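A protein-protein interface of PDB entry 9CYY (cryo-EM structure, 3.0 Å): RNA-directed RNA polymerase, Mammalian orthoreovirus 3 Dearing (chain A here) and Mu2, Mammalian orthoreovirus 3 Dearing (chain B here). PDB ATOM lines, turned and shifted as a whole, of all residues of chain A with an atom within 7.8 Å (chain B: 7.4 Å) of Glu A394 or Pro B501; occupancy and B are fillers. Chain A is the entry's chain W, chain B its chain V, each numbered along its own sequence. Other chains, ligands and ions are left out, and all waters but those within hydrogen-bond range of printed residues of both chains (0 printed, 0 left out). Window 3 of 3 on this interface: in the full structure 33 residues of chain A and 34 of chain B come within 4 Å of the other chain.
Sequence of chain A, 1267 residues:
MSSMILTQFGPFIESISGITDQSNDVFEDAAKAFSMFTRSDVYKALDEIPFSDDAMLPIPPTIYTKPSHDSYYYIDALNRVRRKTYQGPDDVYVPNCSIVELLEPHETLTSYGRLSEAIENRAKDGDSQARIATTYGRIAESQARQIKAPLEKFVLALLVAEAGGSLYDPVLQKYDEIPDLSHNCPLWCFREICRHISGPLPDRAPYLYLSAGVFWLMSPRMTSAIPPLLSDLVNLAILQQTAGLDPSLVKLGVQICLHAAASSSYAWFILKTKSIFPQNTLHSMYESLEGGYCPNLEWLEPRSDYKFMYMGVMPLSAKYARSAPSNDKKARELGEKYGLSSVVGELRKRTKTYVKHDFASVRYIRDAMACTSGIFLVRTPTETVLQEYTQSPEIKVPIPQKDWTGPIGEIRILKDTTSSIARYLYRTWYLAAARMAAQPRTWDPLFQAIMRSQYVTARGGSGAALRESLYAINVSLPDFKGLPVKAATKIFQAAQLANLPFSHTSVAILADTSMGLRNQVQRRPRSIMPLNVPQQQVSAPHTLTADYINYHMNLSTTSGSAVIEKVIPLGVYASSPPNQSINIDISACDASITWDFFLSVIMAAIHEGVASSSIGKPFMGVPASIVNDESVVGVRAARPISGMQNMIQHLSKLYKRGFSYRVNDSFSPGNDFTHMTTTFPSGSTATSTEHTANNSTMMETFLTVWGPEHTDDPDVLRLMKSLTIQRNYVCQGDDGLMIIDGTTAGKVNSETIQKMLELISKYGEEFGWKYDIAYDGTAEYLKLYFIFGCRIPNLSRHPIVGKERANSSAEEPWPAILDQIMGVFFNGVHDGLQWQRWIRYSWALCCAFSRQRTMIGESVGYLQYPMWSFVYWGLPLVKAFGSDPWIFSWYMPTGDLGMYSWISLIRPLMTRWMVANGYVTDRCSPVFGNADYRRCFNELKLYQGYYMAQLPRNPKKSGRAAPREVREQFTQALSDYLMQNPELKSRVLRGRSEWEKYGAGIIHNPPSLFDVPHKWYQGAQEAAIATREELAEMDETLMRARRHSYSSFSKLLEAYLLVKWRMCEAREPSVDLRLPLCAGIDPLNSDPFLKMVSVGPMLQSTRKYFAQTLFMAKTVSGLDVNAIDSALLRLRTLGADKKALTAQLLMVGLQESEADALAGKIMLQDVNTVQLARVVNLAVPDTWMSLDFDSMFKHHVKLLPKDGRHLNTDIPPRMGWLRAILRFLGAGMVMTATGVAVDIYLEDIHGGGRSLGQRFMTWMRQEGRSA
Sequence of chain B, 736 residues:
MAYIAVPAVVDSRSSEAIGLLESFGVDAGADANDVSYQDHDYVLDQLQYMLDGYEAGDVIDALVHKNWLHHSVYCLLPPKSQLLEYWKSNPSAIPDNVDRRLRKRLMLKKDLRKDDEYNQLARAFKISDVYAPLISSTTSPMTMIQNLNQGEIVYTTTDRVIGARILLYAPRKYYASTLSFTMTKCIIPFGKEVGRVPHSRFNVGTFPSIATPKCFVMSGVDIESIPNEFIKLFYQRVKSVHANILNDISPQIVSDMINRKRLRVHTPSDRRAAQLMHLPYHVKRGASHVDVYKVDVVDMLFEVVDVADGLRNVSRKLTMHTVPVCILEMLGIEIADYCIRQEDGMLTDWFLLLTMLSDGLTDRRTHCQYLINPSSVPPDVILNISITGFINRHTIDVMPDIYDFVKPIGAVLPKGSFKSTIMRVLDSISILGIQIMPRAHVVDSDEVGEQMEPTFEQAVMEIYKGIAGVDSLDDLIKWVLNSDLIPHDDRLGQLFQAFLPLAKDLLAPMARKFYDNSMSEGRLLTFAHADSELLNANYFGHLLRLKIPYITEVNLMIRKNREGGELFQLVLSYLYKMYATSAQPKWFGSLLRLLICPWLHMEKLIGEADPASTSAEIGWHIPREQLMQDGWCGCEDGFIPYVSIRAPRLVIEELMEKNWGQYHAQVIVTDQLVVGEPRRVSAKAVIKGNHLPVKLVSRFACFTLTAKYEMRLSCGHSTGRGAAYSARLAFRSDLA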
ATOM      1  N   GLN A 391      12.931  19.821   9.499  1.00  0.00           N
ATOM      2  CA  GLN A 391      13.025  18.609  10.298  1.00  0.00           C
ATOM      3  C   GLN A 391      13.376  17.414   9.418  1.00  0.00           C
ATOM      4  O   GLN A 391      13.242  17.443   8.193  1.00  0.00           O
ATOM      5  CB  GLN A 391      11.720  18.349  11.050  1.00  0.00           C
ATOM      6  CG  GLN A 391      11.143  19.568  11.743  1.00  0.00           C
ATOM      7  CD  GLN A 391      10.199  20.345  10.854  1.00  0.00           C
ATOM      8  OE1 GLN A 391       9.147  19.844  10.458  1.00  0.00           O
ATOM      9  NE2 GLN A 391      10.570  21.579  10.533  1.00  0.00           N
ATOM     10  N   SER A 392      13.834  16.349  10.064  1.00  0.00           N
ATOM     11  CA  SER A 392      14.216  15.125   9.380  1.00  0.00           C
ATOM     12  C   SER A 392      14.033  13.965  10.345  1.00  0.00           C
ATOM     13  O   SER A 392      14.094  14.155  11.566  1.00  0.00           O
ATOM     14  CB  SER A 392      15.666  15.194   8.881  1.00  0.00           C
ATOM     15  OG  SER A 392      16.579  15.239   9.962  1.00  0.00           O
ATOM     16  N   PRO A 393      13.801  12.758   9.838  1.00  0.00           N
ATOM     17  CA  PRO A 393      13.584  11.614  10.726  1.00  0.00           C
ATOM     18  C   PRO A 393      14.840  11.236  11.492  1.00  0.00           C
ATOM     19  O   PRO A 393      15.967  11.485  11.059  1.00  0.00           O
ATOM     20  CB  PRO A 393      13.167  10.488   9.769  1.00  0.00           C
ATOM     21  CG  PRO A 393      12.886  11.149   8.463  1.00  0.00           C
ATOM     22  CD  PRO A 393      13.726  12.372   8.421  1.00  0.00           C
ATOM     23  N   GLU A 394      14.623  10.622  12.650  1.00  0.00           N
ATOM     24  CA  GLU A 394      15.696  10.136  13.512  1.00  0.00           C
ATOM     25  C   GLU A 394      15.589   8.613  13.549  1.00  0.00           C
ATOM     26  O   GLU A 394      14.839   8.045  14.345  1.00  0.00           O
ATOM     27  CB  GLU A 394      15.599  10.747  14.904  1.00  0.00           C
ATOM     28  CG  GLU A 394      16.646  10.243  15.879  1.00  0.00           C
ATOM     29  CD  GLU A 394      16.937  11.236  16.985  1.00  0.00           C
ATOM     30  OE1 GLU A 394      18.084  11.262  17.477  1.00  0.00           O
ATOM     31  OE2 GLU A 394      16.017  11.992  17.363  1.00  0.00           O
ATOM     32  N   ILE A 395      16.346   7.954  12.675  1.00  0.00           N
ATOM     33  CA  ILE A 395      16.320   6.500  12.569  1.00  0.00           C
ATOM     34  C   ILE A 395      17.300   5.910  13.570  1.00  0.00           C
ATOM     35  O   ILE A 395      18.500   5.806  13.291  1.00  0.00           O
ATOM     36  CB  ILE A 395      16.652   6.035  11.140  1.00  0.00           C
ATOM     37  CG1 ILE A 395      15.980   6.940  10.107  1.00  0.00           C
ATOM     38  CG2 ILE A 395      16.227   4.592  10.939  1.00  0.00           C
ATOM     39  CD1 ILE A 395      14.471   6.914  10.160  1.00  0.00           C
ATOM     40  N   LYS A 396      16.799   5.521  14.745  1.00  0.00           N
ATOM     41  CA  LYS A 396      17.676   4.971  15.774  1.00  0.00           C
ATOM     42  C   LYS A 396      18.333   3.676  15.312  1.00  0.00           C
ATOM     43  O   LYS A 396      19.538   3.481  15.504  1.00  0.00           O
ATOM     44  CB  LYS A 396      16.891   4.748  17.066  1.00  0.00           C
ATOM     45  CG  LYS A 396      15.862   5.820  17.360  1.00  0.00           C
ATOM     46  CD  LYS A 396      16.516   7.108  17.823  1.00  0.00           C
ATOM     47  CE  LYS A 396      17.276   6.901  19.119  1.00  0.00           C
ATOM     48  NZ  LYS A 396      16.389   6.372  20.190  1.00  0.00           N
ATOM     49  N   VAL A 397      17.566   2.788  14.690  1.00  0.00           N
ATOM     50  CA  VAL A 397      18.113   1.527  14.197  1.00  0.00           C
ATOM     51  C   VAL A 397      18.029   1.511  12.677  1.00  0.00           C
ATOM     52  O   VAL A 397      16.954   1.248  12.117  1.00  0.00           O
ATOM     53  CB  VAL A 397      17.384   0.320  14.808  1.00  0.00           C
ATOM     54  CG1 VAL A 397      18.005  -0.974  14.313  1.00  0.00           C
ATOM     55  CG2 VAL A 397      17.435   0.389  16.323  1.00  0.00           C
ATOM     56  N   ALA A 591       7.519  14.623   6.879  1.00  0.00           N
ATOM     57  CA  ALA A 591       8.931  14.713   7.227  1.00  0.00           C
ATOM     58  C   ALA A 591       9.525  13.334   7.482  1.00  0.00           C
ATOM     59  O   ALA A 591      10.665  13.058   7.091  1.00  0.00           O
ATOM     60  CB  ALA A 591       9.117  15.612   8.447  1.00  0.00           C
ATOM     61  N   SER A 592       8.766  12.454   8.140  1.00  0.00           N
ATOM     62  CA  SER A 592       9.273  11.122   8.450  1.00  0.00           C
ATOM     63  C   SER A 592       9.487  10.300   7.186  1.00  0.00           C
ATOM     64  O   SER A 592      10.421   9.492   7.112  1.00  0.00           O
ATOM     65  CB  SER A 592       8.314  10.406   9.399  1.00  0.00           C
ATOM     66  OG  SER A 592       7.072  10.153   8.768  1.00  0.00           O
ATOM     67  N   THR A 594      10.986   9.445   4.015  1.00  0.00           N
ATOM     68  CA  THR A 594      12.226   9.875   3.378  1.00  0.00           C
ATOM     69  C   THR A 594      12.854   8.714   2.623  1.00  0.00           C
ATOM     70  O   THR A 594      12.433   7.561   2.750  1.00  0.00           O
ATOM     71  CB  THR A 594      13.233  10.430   4.394  1.00  0.00           C
ATOM     72  OG1 THR A 594      13.359   9.519   5.492  1.00  0.00           O
ATOM     73  CG2 THR A 594      12.810  11.802   4.899  1.00  0.00           C
ATOM     74  N   ASP A 596      15.761   7.413   3.064  1.00  0.00           N
ATOM     75  CA  ASP A 596      16.679   6.572   3.825  1.00  0.00           C
ATOM     76  C   ASP A 596      16.099   5.184   4.068  1.00  0.00           C
ATOM     77  O   ASP A 596      16.804   4.177   3.936  1.00  0.00           O
ATOM     78  CB  ASP A 596      17.029   7.247   5.150  1.00  0.00           C
ATOM     79  CG  ASP A 596      17.759   6.321   6.098  1.00  0.00           C
ATOM     80  OD1 ASP A 596      18.993   6.184   5.966  1.00  0.00           O
ATOM     81  OD2 ASP A 596      17.099   5.732   6.979  1.00  0.00           O
ATOM     82  N   GLY A 764       7.981   2.406  17.595  1.00  0.00           N
ATOM     83  CA  GLY A 764       7.970   3.520  16.663  1.00  0.00           C
ATOM     84  C   GLY A 764       9.321   4.198  16.502  1.00  0.00           C
ATOM     85  O   GLY A 764       9.713   4.551  15.383  1.00  0.00           O
ATOM     86  N   GLU A 765      10.052   4.406  17.607  1.00  0.00           N
ATOM     87  CA  GLU A 765      11.266   5.227  17.462  1.00  0.00           C
ATOM     88  C   GLU A 765      12.307   4.586  16.543  1.00  0.00           C
ATOM     89  O   GLU A 765      13.120   5.304  15.951  1.00  0.00           O
ATOM     90  CB  GLU A 765      11.962   5.610  18.780  1.00  0.00           C
ATOM     91  CG  GLU A 765      11.243   6.563  19.729  1.00  0.00           C
ATOM     92  CD  GLU A 765      10.282   5.869  20.613  1.00  0.00           C
ATOM     93  OE1 GLU A 765      10.260   4.637  20.510  1.00  0.00           O
ATOM     94  OE2 GLU A 765       9.569   6.533  21.395  1.00  0.00           O
ATOM     95  N   GLU A 766      12.325   3.252  16.413  1.00  0.00           N
ATOM     96  CA  GLU A 766      13.399   2.627  15.635  1.00  0.00           C
ATOM     97  C   GLU A 766      13.439   3.151  14.206  1.00  0.00           C
ATOM     98  O   GLU A 766      14.491   3.594  13.729  1.00  0.00           O
ATOM     99  CB  GLU A 766      13.276   1.102  15.615  1.00  0.00           C
ATOM    100  CG  GLU A 766      13.831   0.405  16.841  1.00  0.00           C
ATOM    101  CD  GLU A 766      12.896   0.493  18.008  1.00  0.00           C
ATOM    102  OE1 GLU A 766      13.367   0.588  19.161  1.00  0.00           O
ATOM    103  OE2 GLU A 766      11.678   0.443  17.755  1.00  0.00           O
ATOM    104  N   PHE A 767      12.309   3.115  13.506  1.00  0.00           N
ATOM    105  CA  PHE A 767      12.219   3.710  12.182  1.00  0.00           C
ATOM    106  C   PHE A 767      11.794   5.171  12.250  1.00  0.00           C
ATOM    107  O   PHE A 767      11.598   5.808  11.211  1.00  0.00           O
ATOM    108  CB  PHE A 767      11.275   2.906  11.290  1.00  0.00           C
ATOM    109  CG  PHE A 767       9.915   2.694  11.877  1.00  0.00           C
ATOM    110  CD1 PHE A 767       9.682   1.638  12.739  1.00  0.00           C
ATOM    111  CD2 PHE A 767       8.864   3.532  11.551  1.00  0.00           C
ATOM    112  CE1 PHE A 767       8.434   1.432  13.282  1.00  0.00           C
ATOM    113  CE2 PHE A 767       7.612   3.327  12.087  1.00  0.00           C
ATOM    114  CZ  PHE A 767       7.397   2.275  12.955  1.00  0.00           C
ATOM    115  N   GLY A 768      11.646   5.711  13.455  1.00  0.00           N
ATOM    116  CA  GLY A 768      11.561   7.153  13.594  1.00  0.00           C
ATOM    117  C   GLY A 768      10.208   7.749  13.289  1.00  0.00           C
ATOM    118  O   GLY A 768      10.131   8.817  12.668  1.00  0.00           O
ATOM    119  N   TRP A 769       9.135   7.087  13.707  1.00  0.00           N
ATOM    120  CA  TRP A 769       7.788   7.621  13.583  1.00  0.00           C
ATOM    121  C   TRP A 769       7.337   8.081  14.959  1.00  0.00           C
ATOM    122  O   TRP A 769       7.329   7.292  15.909  1.00  0.00           O
ATOM    123  CB  TRP A 769       6.826   6.576  13.018  1.00  0.00           C
ATOM    124  CG  TRP A 769       6.668   6.655  11.535  1.00  0.00           C
ATOM    125  CD1 TRP A 769       7.462   7.337  10.664  1.00  0.00           C
ATOM    126  CD2 TRP A 769       5.660   6.016  10.743  1.00  0.00           C
ATOM    127  NE1 TRP A 769       7.008   7.172   9.379  1.00  0.00           N
ATOM    128  CE2 TRP A 769       5.902   6.364   9.400  1.00  0.00           C
ATOM    129  CE3 TRP A 769       4.574   5.188  11.039  1.00  0.00           C
ATOM    130  CZ2 TRP A 769       5.100   5.912   8.356  1.00  0.00           C
ATOM    131  CZ3 TRP A 769       3.780   4.740  10.000  1.00  0.00           C
ATOM    132  CH2 TRP A 769       4.046   5.102   8.677  1.00  0.00           C
ATOM    133  N   PHE B 456      33.008  18.958  18.237  1.00  0.00           N
ATOM    134  CA  PHE B 456      32.201  17.742  18.221  1.00  0.00           C
ATOM    135  C   PHE B 456      32.959  16.542  18.770  1.00  0.00           C
ATOM    136  O   PHE B 456      32.368  15.665  19.407  1.00  0.00           O
ATOM    137  CB  PHE B 456      31.716  17.461  16.797  1.00  0.00           C
ATOM    138  CG  PHE B 456      30.446  16.663  16.740  1.00  0.00           C
ATOM    139  CD1 PHE B 456      29.292  17.133  17.342  1.00  0.00           C
ATOM    140  CD2 PHE B 456      30.404  15.446  16.083  1.00  0.00           C
ATOM    141  CE1 PHE B 456      28.120  16.405  17.291  1.00  0.00           C
ATOM    142  CE2 PHE B 456      29.234  14.713  16.029  1.00  0.00           C
ATOM    143  CZ  PHE B 456      28.092  15.194  16.634  1.00  0.00           C
ATOM    144  N   ILE B 463      30.262  10.330  25.996  1.00  0.00           N
ATOM    145  CA  ILE B 463      29.199   9.333  25.929  1.00  0.00           C
ATOM    146  C   ILE B 463      29.371   8.300  27.036  1.00  0.00           C
ATOM    147  O   ILE B 463      28.418   7.603  27.405  1.00  0.00           O
ATOM    148  CB  ILE B 463      29.171   8.685  24.529  1.00  0.00           C
ATOM    149  CG1 ILE B 463      28.941   9.751  23.458  1.00  0.00           C
ATOM    150  CG2 ILE B 463      28.085   7.628  24.431  1.00  0.00           C
ATOM    151  CD1 ILE B 463      27.488  10.122  23.261  1.00  0.00           C
ATOM    152  N   LEU B 495      25.707   2.392  21.368  1.00  0.00           N
ATOM    153  CA  LEU B 495      26.519   3.591  21.211  1.00  0.00           C
ATOM    154  C   LEU B 495      25.934   4.505  20.143  1.00  0.00           C
ATOM    155  O   LEU B 495      25.940   5.731  20.289  1.00  0.00           O
ATOM    156  CB  LEU B 495      27.956   3.202  20.875  1.00  0.00           C
ATOM    157  CG  LEU B 495      28.948   4.352  20.745  1.00  0.00           C
ATOM    158  CD1 LEU B 495      29.071   5.082  22.066  1.00  0.00           C
ATOM    159  CD2 LEU B 495      30.291   3.818  20.311  1.00  0.00           C
ATOM    160  N   PHE B 496      25.421   3.923  19.056  1.00  0.00           N
ATOM    161  CA  PHE B 496      24.728   4.720  18.049  1.00  0.00           C
ATOM    162  C   PHE B 496      23.460   5.350  18.608  1.00  0.00           C
ATOM    163  O   PHE B 496      23.132   6.493  18.266  1.00  0.00           O
ATOM    164  CB  PHE B 496      24.394   3.861  16.832  1.00  0.00           C
ATOM    165  CG  PHE B 496      23.859   4.644  15.669  1.00  0.00           C
ATOM    166  CD1 PHE B 496      24.684   5.483  14.943  1.00  0.00           C
ATOM    167  CD2 PHE B 496      22.527   4.547  15.307  1.00  0.00           C
ATOM    168  CE1 PHE B 496      24.193   6.206  13.874  1.00  0.00           C
ATOM    169  CE2 PHE B 496      22.030   5.266  14.240  1.00  0.00           C
ATOM    170  CZ  PHE B 496      22.864   6.097  13.523  1.00  0.00           C
ATOM    171  N   GLN B 497      22.726   4.614  19.449  1.00  0.00           N
ATOM    172  CA  GLN B 497      21.558   5.187  20.111  1.00  0.00           C
ATOM    173  C   GLN B 497      21.939   6.433  20.895  1.00  0.00           C
ATOM    174  O   GLN B 497      21.227   7.443  20.862  1.00  0.00           O
ATOM    175  CB  GLN B 497      20.915   4.164  21.049  1.00  0.00           C
ATOM    176  CG  GLN B 497      20.376   2.920  20.378  1.00  0.00           C
ATOM    177  CD  GLN B 497      19.240   3.215  19.431  1.00  0.00           C
ATOM    178  OE1 GLN B 497      19.443   3.335  18.226  1.00  0.00           O
ATOM    179  NE2 GLN B 497      18.034   3.335  19.971  1.00  0.00           N
ATOM    180  N   ALA B 498      23.058   6.372  21.612  1.00  0.00           N
ATOM    181  CA  ALA B 498      23.511   7.535  22.372  1.00  0.00           C
ATOM    182  C   ALA B 498      24.027   8.645  21.459  1.00  0.00           C
ATOM    183  O   ALA B 498      23.861   9.831  21.764  1.00  0.00           O
ATOM    184  CB  ALA B 498      24.591   7.122  23.370  1.00  0.00           C
ATOM    185  N   PHE B 499      24.655   8.277  20.340  1.00  0.00           N
ATOM    186  CA  PHE B 499      25.319   9.258  19.486  1.00  0.00           C
ATOM    187  C   PHE B 499      24.325  10.059  18.655  1.00  0.00           C
ATOM    188  O   PHE B 499      24.529  11.256  18.421  1.00  0.00           O
ATOM    189  CB  PHE B 499      26.319   8.549  18.574  1.00  0.00           C
ATOM    190  CG  PHE B 499      26.869   9.417  17.479  1.00  0.00           C
ATOM    191  CD1 PHE B 499      27.837  10.367  17.748  1.00  0.00           C
ATOM    192  CD2 PHE B 499      26.418   9.278  16.177  1.00  0.00           C
ATOM    193  CE1 PHE B 499      28.344  11.162  16.740  1.00  0.00           C
ATOM    194  CE2 PHE B 499      26.921  10.070  15.165  1.00  0.00           C
ATOM    195  CZ  PHE B 499      27.885  11.014  15.448  1.00  0.00           C
ATOM    196  N   LEU B 500      23.257   9.414  18.185  1.00  0.00           N
ATOM    197  CA  LEU B 500      22.352  10.060  17.234  1.00  0.00           C
ATOM    198  C   LEU B 500      21.796  11.394  17.717  1.00  0.00           C
ATOM    199  O   LEU B 500      21.766  12.346  16.916  1.00  0.00           O
ATOM    200  CB  LEU B 500      21.221   9.093  16.869  1.00  0.00           C
ATOM    201  CG  LEU B 500      20.514   9.376  15.544  1.00  0.00           C
ATOM    202  CD1 LEU B 500      21.526   9.680  14.453  1.00  0.00           C
ATOM    203  CD2 LEU B 500      19.633   8.206  15.148  1.00  0.00           C
ATOM    204  N   PRO B 501      21.331  11.545  18.967  1.00  0.00           N
ATOM    205  CA  PRO B 501      20.808  12.861  19.377  1.00  0.00           C
ATOM    206  C   PRO B 501      21.801  13.994  19.194  1.00  0.00           C
ATOM    207  O   PRO B 501      21.454  15.023  18.603  1.00  0.00           O
ATOM    208  CB  PRO B 501      20.451  12.642  20.852  1.00  0.00           C
ATOM    209  CG  PRO B 501      20.153  11.200  20.947  1.00  0.00           C
ATOM    210  CD  PRO B 501      21.123  10.535  20.020  1.00  0.00           C
ATOM    211  N   LEU B 502      23.039  13.821  19.665  1.00  0.00           N
ATOM    212  CA  LEU B 502      24.023  14.896  19.580  1.00  0.00           C
ATOM    213  C   LEU B 502      24.290  15.294  18.135  1.00  0.00           C
ATOM    214  O   LEU B 502      24.367  16.485  17.815  1.00  0.00           O
ATOM    215  CB  LEU B 502      25.323  14.469  20.260  1.00  0.00           C
ATOM    216  CG  LEU B 502      25.256  14.247  21.770  1.00  0.00           C
ATOM    217  CD1 LEU B 502      26.576  13.695  22.282  1.00  0.00           C
ATOM    218  CD2 LEU B 502      24.896  15.538  22.483  1.00  0.00           C
ATOM    219  N   ALA B 503      24.437  14.309  17.249  1.00  0.00           N
ATOM    220  CA  ALA B 503      24.659  14.615  15.841  1.00  0.00           C
ATOM    221  C   ALA B 503      23.432  15.264  15.217  1.00  0.00           C
ATOM    222  O   ALA B 503      23.543  15.992  14.224  1.00  0.00           O
ATOM    223  CB  ALA B 503      25.041  13.346  15.081  1.00  0.00           C
ATOM    224  N   LYS B 504      22.253  15.017  15.784  1.00  0.00           N
ATOM    225  CA  LYS B 504      21.016  15.516  15.201  1.00  0.00           C
ATOM    226  C   LYS B 504      20.654  16.932  15.635  1.00  0.00           C
ATOM    227  O   LYS B 504      20.136  17.695  14.812  1.00  0.00           O
ATOM    228  CB  LYS B 504      19.859  14.574  15.543  1.00  0.00           C
ATOM    229  CG  LYS B 504      19.493  13.618  14.422  1.00  0.00           C
ATOM    230  CD  LYS B 504      18.943  14.370  13.225  1.00  0.00           C
ATOM    231  CE  LYS B 504      17.486  14.738  13.442  1.00  0.00           C
ATOM    232  NZ  LYS B 504      16.825  15.198  12.192  1.00  0.00           N
ATOM    233  N   ASP B 505      20.904  17.310  16.889  1.00  0.00           N
ATOM    234  CA  ASP B 505      20.405  18.573  17.419  1.00  0.00           C
ATOM    235  C   ASP B 505      21.485  19.617  17.684  1.00  0.00           C
ATOM    236  O   ASP B 505      21.147  20.781  17.920  1.00  0.00           O
ATOM    237  CB  ASP B 505      19.593  18.319  18.697  1.00  0.00           C
ATOM    238  CG  ASP B 505      20.422  17.715  19.813  1.00  0.00           C
ATOM    239  OD1 ASP B 505      21.621  17.448  19.595  1.00  0.00           O
ATOM    240  OD2 ASP B 505      19.872  17.502  20.913  1.00  0.00           O
ATOM    241  N   LEU B 506      22.764  19.245  17.656  1.00  0.00           N
ATOM    242  CA  LEU B 506      23.829  20.234  17.806  1.00  0.00           C
ATOM    243  C   LEU B 506      24.490  20.563  16.475  1.00  0.00           C
ATOM    244  O   LEU B 506      24.591  21.735  16.099  1.00  0.00           O
ATOM    245  CB  LEU B 506      24.894  19.755  18.799  1.00  0.00           C
ATOM    246  CG  LEU B 506      24.747  20.068  20.291  1.00  0.00           C
ATOM    247  CD1 LEU B 506      23.480  19.494  20.890  1.00  0.00           C
ATOM    248  CD2 LEU B 506      25.969  19.566  21.047  1.00  0.00           C
ATOM    249  N   LEU B 507      24.946  19.536  15.759  1.00  0.00           N
ATOM    250  CA  LEU B 507      25.738  19.770  14.557  1.00  0.00           C
ATOM    251  C   LEU B 507      24.892  20.350  13.431  1.00  0.00           C
ATOM    252  O   LEU B 507      25.384  21.148  12.624  1.00  0.00           O
ATOM    253  CB  LEU B 507      26.407  18.470  14.115  1.00  0.00           C
ATOM    254  CG  LEU B 507      27.307  18.544  12.883  1.00  0.00           C
ATOM    255  CD1 LEU B 507      28.645  19.163  13.245  1.00  0.00           C
ATOM    256  CD2 LEU B 507      27.499  17.163  12.281  1.00  0.00           C
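The backbone carbonyl oxygen of Pro B501 lies close to the side-chain carboxylate of Asp B505. The backbone carbonyl oxygen (O) of Glu A766 is in hydrogen-bond range of the backbone NH (N) of Lys A396, at 3.2 Å.
Hydrophobic or aromatic side chains of chain B within 4 Å of the printed part of chain A: Phe B496 and Leu B500. Among the printed residues, 9 pairs touch across the chains.
Pro A393 touches Lys B504. Glu A394 touches Leu B500 (OE1 to CG, 3.6 Å). Glu A394 touches Pro B501. O of Ile A395 touches CE2 of Phe B496, 3.7 Å away. Leu B500 touches Ile A395. Lys A396 touches Phe B496. Leu B500 touches Lys A396.
Glu A394 touches just these residues of chain B: Leu B500 (3.6 Å) and Pro B501 (3.6 Å). Pro B501 touches just one residue of chain A: Glu A394 (3.6 Å). Of the printed residues of chain A, Gln B497 touches Lys A396 (2.7 Å). Of the printed residues of chain B, Ser A392 touches Lys B504 (2.2 Å). Phe A767 touches none of the printed residues of chain B. Phe B499 touches none of the printed residues of chain A. The nearest residue of chain B that does not touch Glu A394 is Lys B504 (4.1 Å). The nearest residue of chain A that does not touch Pro B501 is Lys A396 (5.4 Å).
The side-chain amide oxygen (OE1) of Gln B497 sits close to the backbone carbonyl oxygen (O) of Lys A396, at 2.7 Å. The side-chain amino group of Lys B504 is in hydrogen-bond range of the backbone carbonyl oxygen of Ser A392.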
